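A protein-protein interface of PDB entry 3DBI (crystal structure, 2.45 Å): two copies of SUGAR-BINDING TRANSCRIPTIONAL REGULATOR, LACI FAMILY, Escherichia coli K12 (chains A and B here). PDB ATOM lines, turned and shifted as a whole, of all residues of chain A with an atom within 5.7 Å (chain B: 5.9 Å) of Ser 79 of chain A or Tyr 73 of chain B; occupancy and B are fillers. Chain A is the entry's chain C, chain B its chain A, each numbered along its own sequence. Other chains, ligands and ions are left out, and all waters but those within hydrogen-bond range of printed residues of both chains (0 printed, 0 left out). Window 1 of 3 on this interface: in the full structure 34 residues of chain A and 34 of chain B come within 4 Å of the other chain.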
ATOM      1  N   GLY A  75      27.656 -10.944 -17.432  1.00  0.00           N
ATOM      2  CA  GLY A  75      26.672 -11.998 -17.658  1.00  0.00           C
ATOM      3  C   GLY A  75      25.909 -11.763 -18.957  1.00  0.00           C
ATOM      4  O   GLY A  75      26.302 -10.933 -19.790  1.00  0.00           O
ATOM      5  N   ILE A  76      24.802 -12.477 -19.129  1.00  0.00           N
ATOM      6  CA  ILE A  76      24.036 -12.370 -20.370  1.00  0.00           C
ATOM      7  C   ILE A  76      22.715 -11.605 -20.202  1.00  0.00           C
ATOM      8  O   ILE A  76      21.892 -11.576 -21.128  1.00  0.00           O
ATOM      9  CB  ILE A  76      23.822 -13.758 -21.043  1.00  0.00           C
ATOM     10  CG1 ILE A  76      22.970 -14.675 -20.154  1.00  0.00           C
ATOM     11  CG2 ILE A  76      25.180 -14.396 -21.381  1.00  0.00           C
ATOM     12  CD1 ILE A  76      22.415 -15.930 -20.851  1.00  0.00           C
ATOM     13  N   TYR A  77      22.538 -10.976 -19.036  1.00  0.00           N
ATOM     14  CA  TYR A  77      21.288 -10.303 -18.689  1.00  0.00           C
ATOM     15  C   TYR A  77      20.854  -9.294 -19.737  1.00  0.00           C
ATOM     16  O   TYR A  77      19.739  -9.370 -20.240  1.00  0.00           O
ATOM     17  CB  TYR A  77      21.389  -9.585 -17.344  1.00  0.00           C
ATOM     18  CG  TYR A  77      21.549 -10.466 -16.130  1.00  0.00           C
ATOM     19  CD1 TYR A  77      20.439 -11.040 -15.508  1.00  0.00           C
ATOM     20  CD2 TYR A  77      22.810 -10.703 -15.581  1.00  0.00           C
ATOM     21  CE1 TYR A  77      20.587 -11.839 -14.378  1.00  0.00           C
ATOM     22  CE2 TYR A  77      22.967 -11.502 -14.459  1.00  0.00           C
ATOM     23  CZ  TYR A  77      21.851 -12.065 -13.861  1.00  0.00           C
ATOM     24  OH  TYR A  77      22.002 -12.859 -12.752  1.00  0.00           O
ATOM     25  N   PHE A  78      21.734  -8.355 -20.073  1.00  0.00           N
ATOM     26  CA  PHE A  78      21.350  -7.268 -20.973  1.00  0.00           C
ATOM     27  C   PHE A  78      21.089  -7.723 -22.408  1.00  0.00           C
ATOM     28  O   PHE A  78      20.096  -7.318 -23.005  1.00  0.00           O
ATOM     29  CB  PHE A  78      22.354  -6.110 -20.962  1.00  0.00           C
ATOM     30  CG  PHE A  78      21.981  -4.994 -21.892  1.00  0.00           C
ATOM     31  CD1 PHE A  78      21.039  -4.037 -21.505  1.00  0.00           C
ATOM     32  CD2 PHE A  78      22.544  -4.911 -23.168  1.00  0.00           C
ATOM     33  CE1 PHE A  78      20.675  -3.007 -22.371  1.00  0.00           C
ATOM     34  CE2 PHE A  78      22.182  -3.893 -24.040  1.00  0.00           C
ATOM     35  CZ  PHE A  78      21.245  -2.934 -23.641  1.00  0.00           C
ATOM     36  N   SER A  79      21.978  -8.544 -22.959  1.00  0.00           N
ATOM     37  CA  SER A  79      21.811  -9.003 -24.339  1.00  0.00           C
ATOM     38  C   SER A  79      20.555  -9.860 -24.525  1.00  0.00           C
ATOM     39  O   SER A  79      19.854  -9.696 -25.527  1.00  0.00           O
ATOM     40  CB  SER A  79      23.072  -9.687 -24.895  1.00  0.00           C
ATOM     41  OG  SER A  79      23.837 -10.299 -23.880  1.00  0.00           O
ATOM     42  N   GLU A  80      20.244 -10.719 -23.552  1.00  0.00           N
ATOM     43  CA  GLU A  80      18.989 -11.481 -23.577  1.00  0.00           C
ATOM     44  C   GLU A  80      17.774 -10.565 -23.448  1.00  0.00           C
ATOM     45  O   GLU A  80      16.781 -10.741 -24.164  1.00  0.00           O
ATOM     46  CB  GLU A  80      18.939 -12.560 -22.485  1.00  0.00           C
ATOM     47  CG  GLU A  80      19.847 -13.763 -22.708  1.00  0.00           C
ATOM     48  CD  GLU A  80      19.475 -14.583 -23.932  1.00  0.00           C
ATOM     49  OE1 GLU A  80      18.351 -15.134 -23.974  1.00  0.00           O
ATOM     50  OE2 GLU A  80      20.317 -14.689 -24.850  1.00  0.00           O
ATOM     51  N   LEU A  81      17.863  -9.585 -22.555  1.00  0.00           N
ATOM     52  CA  LEU A  81      16.801  -8.591 -22.397  1.00  0.00           C
ATOM     53  C   LEU A  81      16.550  -7.876 -23.715  1.00  0.00           C
ATOM     54  O   LEU A  81      15.397  -7.701 -24.110  1.00  0.00           O
ATOM     55  CB  LEU A  81      17.139  -7.570 -21.303  1.00  0.00           C
ATOM     56  CG  LEU A  81      16.170  -6.410 -21.024  1.00  0.00           C
ATOM     57  CD1 LEU A  81      14.774  -6.909 -20.676  1.00  0.00           C
ATOM     58  CD2 LEU A  81      16.699  -5.518 -19.908  1.00  0.00           C
ATOM     59  N   LEU A  82      17.636  -7.490 -24.388  1.00  0.00           N
ATOM     60  CA  LEU A  82      17.570  -6.805 -25.672  1.00  0.00           C
ATOM     61  C   LEU A  82      16.924  -7.662 -26.759  1.00  0.00           C
ATOM     62  O   LEU A  82      15.995  -7.212 -27.441  1.00  0.00           O
ATOM     63  CB  LEU A  82      18.960  -6.369 -26.111  1.00  0.00           C
ATOM     64  CG  LEU A  82      18.961  -5.392 -27.280  1.00  0.00           C
ATOM     65  CD1 LEU A  82      19.803  -4.198 -26.900  1.00  0.00           C
ATOM     66  CD2 LEU A  82      19.440  -6.054 -28.579  1.00  0.00           C
ATOM     67  N   PHE A  83      17.432  -8.882 -26.914  1.00  0.00           N
ATOM     68  CA  PHE A  83      16.904  -9.843 -27.872  1.00  0.00           C
ATOM     69  C   PHE A  83      15.392 -10.013 -27.707  1.00  0.00           C
ATOM     70  O   PHE A  83      14.642  -9.779 -28.649  1.00  0.00           O
ATOM     71  CB  PHE A  83      17.620 -11.184 -27.711  1.00  0.00           C
ATOM     72  CG  PHE A  83      17.159 -12.242 -28.670  1.00  0.00           C
ATOM     73  CD1 PHE A  83      17.656 -12.279 -29.972  1.00  0.00           C
ATOM     74  CD2 PHE A  83      16.236 -13.214 -28.273  1.00  0.00           C
ATOM     75  CE1 PHE A  83      17.232 -13.263 -30.870  1.00  0.00           C
ATOM     76  CE2 PHE A  83      15.802 -14.200 -29.159  1.00  0.00           C
ATOM     77  CZ  PHE A  83      16.305 -14.227 -30.458  1.00  0.00           C
ATOM     78  N   HIS A  84      14.958 -10.381 -26.501  1.00  0.00           N
ATOM     79  CA  HIS A  84      13.542 -10.622 -26.218  1.00  0.00           C
ATOM     80  C   HIS A  84      12.661  -9.389 -26.312  1.00  0.00           C
ATOM     81  O   HIS A  84      11.526  -9.495 -26.758  1.00  0.00           O
ATOM     82  CB  HIS A  84      13.358 -11.265 -24.849  1.00  0.00           C
ATOM     83  CG  HIS A  84      13.819 -12.686 -24.784  1.00  0.00           C
ATOM     84  ND1 HIS A  84      15.141 -13.030 -24.611  1.00  0.00           N
ATOM     85  CD2 HIS A  84      13.135 -13.850 -24.869  1.00  0.00           C
ATOM     86  CE1 HIS A  84      15.252 -14.346 -24.592  1.00  0.00           C
ATOM     87  NE2 HIS A  84      14.049 -14.867 -24.747  1.00  0.00           N
ATOM     88  N   THR B  71      23.328 -12.455 -33.948  1.00  0.00           N
ATOM     89  CA  THR B  71      24.780 -12.371 -33.849  1.00  0.00           C
ATOM     90  C   THR B  71      25.268 -11.867 -32.484  1.00  0.00           C
ATOM     91  O   THR B  71      26.470 -11.656 -32.302  1.00  0.00           O
ATOM     92  CB  THR B  71      25.379 -11.476 -34.963  1.00  0.00           C
ATOM     93  OG1 THR B  71      24.698 -10.215 -34.988  1.00  0.00           O
ATOM     94  CG2 THR B  71      25.279 -12.141 -36.342  1.00  0.00           C
ATOM     95  N   LEU B  72      24.355 -11.663 -31.532  1.00  0.00           N
ATOM     96  CA  LEU B  72      24.775 -11.458 -30.137  1.00  0.00           C
ATOM     97  C   LEU B  72      25.427 -12.756 -29.667  1.00  0.00           C
ATOM     98  O   LEU B  72      24.921 -13.822 -29.970  1.00  0.00           O
ATOM     99  CB  LEU B  72      23.625 -11.037 -29.196  1.00  0.00           C
ATOM    100  CG  LEU B  72      22.117 -11.104 -29.449  1.00  0.00           C
ATOM    101  CD1 LEU B  72      21.375 -11.086 -28.138  1.00  0.00           C
ATOM    102  CD2 LEU B  72      21.638  -9.969 -30.333  1.00  0.00           C
ATOM    103  N   TYR B  73      26.558 -12.660 -28.967  1.00  0.00           N
ATOM    104  CA  TYR B  73      27.418 -13.803 -28.546  1.00  0.00           C
ATOM    105  C   TYR B  73      28.326 -14.380 -29.648  1.00  0.00           C
ATOM    106  O   TYR B  73      29.208 -15.194 -29.353  1.00  0.00           O
ATOM    107  CB  TYR B  73      26.662 -14.939 -27.798  1.00  0.00           C
ATOM    108  CG  TYR B  73      25.565 -14.466 -26.859  1.00  0.00           C
ATOM    109  CD1 TYR B  73      24.228 -14.812 -27.091  1.00  0.00           C
ATOM    110  CD2 TYR B  73      25.857 -13.655 -25.756  1.00  0.00           C
ATOM    111  CE1 TYR B  73      23.215 -14.369 -26.259  1.00  0.00           C
ATOM    112  CE2 TYR B  73      24.851 -13.212 -24.912  1.00  0.00           C
ATOM    113  CZ  TYR B  73      23.530 -13.574 -25.170  1.00  0.00           C
ATOM    114  OH  TYR B  73      22.524 -13.139 -24.342  1.00  0.00           O
ATOM    115  N   HIS B  74      28.126 -13.959 -30.899  1.00  0.00           N
ATOM    116  CA  HIS B  74      29.057 -14.317 -31.976  1.00  0.00           C
ATOM    117  C   HIS B  74      30.179 -13.281 -32.053  1.00  0.00           C
ATOM    118  O   HIS B  74      30.176 -12.388 -32.914  1.00  0.00           O
ATOM    119  CB  HIS B  74      28.346 -14.471 -33.325  1.00  0.00           C
ATOM    120  CG  HIS B  74      29.204 -15.099 -34.380  1.00  0.00           C
ATOM    121  ND1 HIS B  74      29.605 -16.417 -34.325  1.00  0.00           N
ATOM    122  CD2 HIS B  74      29.752 -14.587 -35.507  1.00  0.00           C
ATOM    123  CE1 HIS B  74      30.359 -16.691 -35.375  1.00  0.00           C
ATOM    124  NE2 HIS B  74      30.463 -15.597 -36.107  1.00  0.00           N
ATOM    125  N   GLY B  75      31.131 -13.400 -31.130  1.00  0.00           N
ATOM    126  CA  GLY B  75      32.127 -12.358 -30.923  1.00  0.00           C
ATOM    127  C   GLY B  75      31.471 -11.118 -30.334  1.00  0.00           C
ATOM    128  O   GLY B  75      30.316 -11.148 -29.896  1.00  0.00           O
ATOM    129  N   ILE B  76      32.197 -10.009 -30.340  1.00  0.00           N
ATOM    130  CA  ILE B  76      31.692  -8.810 -29.694  1.00  0.00           C
ATOM    131  C   ILE B  76      31.204  -7.760 -30.703  1.00  0.00           C
ATOM    132  O   ILE B  76      30.969  -6.610 -30.332  1.00  0.00           O
ATOM    133  CB  ILE B  76      32.731  -8.231 -28.681  1.00  0.00           C
ATOM    134  CG1 ILE B  76      34.025  -7.787 -29.390  1.00  0.00           C
ATOM    135  CG2 ILE B  76      33.032  -9.265 -27.577  1.00  0.00           C
ATOM    136  CD1 ILE B  76      34.912  -6.842 -28.562  1.00  0.00           C
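Printed residues of chain A that touch a printed residue of chain B: Ile 76, Ser 79, Glu 80 and Phe 83. Hydrophobic or aromatic side chains of chain A within 4 Å of the printed part of chain B: Ile 76 and Phe 83. Hydrophobic or aromatic side chains of chain B within 4 Å of the printed part of chain A: Leu 72 and Tyr 73. Among the printed residues, no Asp or Glu carboxylate lies within 4 Å of a Lys or Arg side-chain nitrogen of the other chain.
A ring nitrogen (ND1) of His 84 of chain A is in hydrogen-bond range of the backbone carbonyl oxygen of Glu 80 of chain A.
Of the printed residues of chain B, Ile 76 of chain A touches Tyr 73 (3.6 Å). Phe 78 of chain A touches none of the printed residues of chain B. Of chain B, only Leu 72 and Tyr 73 come within 4 Å of Ser 79 of chain A. Of the printed residues of chain B, Glu 80 of chain A touches Tyr 73 (2.7 Å). His 84 of chain A touches none of the printed residues of chain B. Printed residues of chain A within 4 Å of Leu 72 of chain B: Ser 79 and Phe 83. Tyr 73 of chain B touches three residues of chain A. The nearest printed residue of chain B that does not touch Ser 79 of chain A is Thr 71 of chain B (8.2 Å). The nearest printed residue of chain A that does not touch Tyr 73 of chain B is Tyr 77 of chain A (5.7 Å). The nearest printed residue of chain B that does not touch Ile 76 of chain A is Leu 72 of chain B (7.0 Å).
OH of Tyr 73 of chain B sits at hydrogen-bond distance from OG of Ser 79 of chain A, 3.2 Å away. The side-chain carboxylate (OE2) of Glu 80 of chain A lies within hydrogen-bond range of the side-chain hydroxyl (OH) of Tyr 73 of chain B, at 2.7 Å.
Among the printed residues, pairs that only touch across the chains: Ser 79 of chain A with Leu 72 of chain B (3.3 Å), Ile 76 of chain A with Tyr 73 of chain B (3.6 Å) and Phe 83 of chain A with Leu 72 of chain B (3.8 Å).
2 positions are printed for both chains. Of the 5 pairs that touch across the chains among the printed residues, none has its exchanged pair printed and touching as well.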
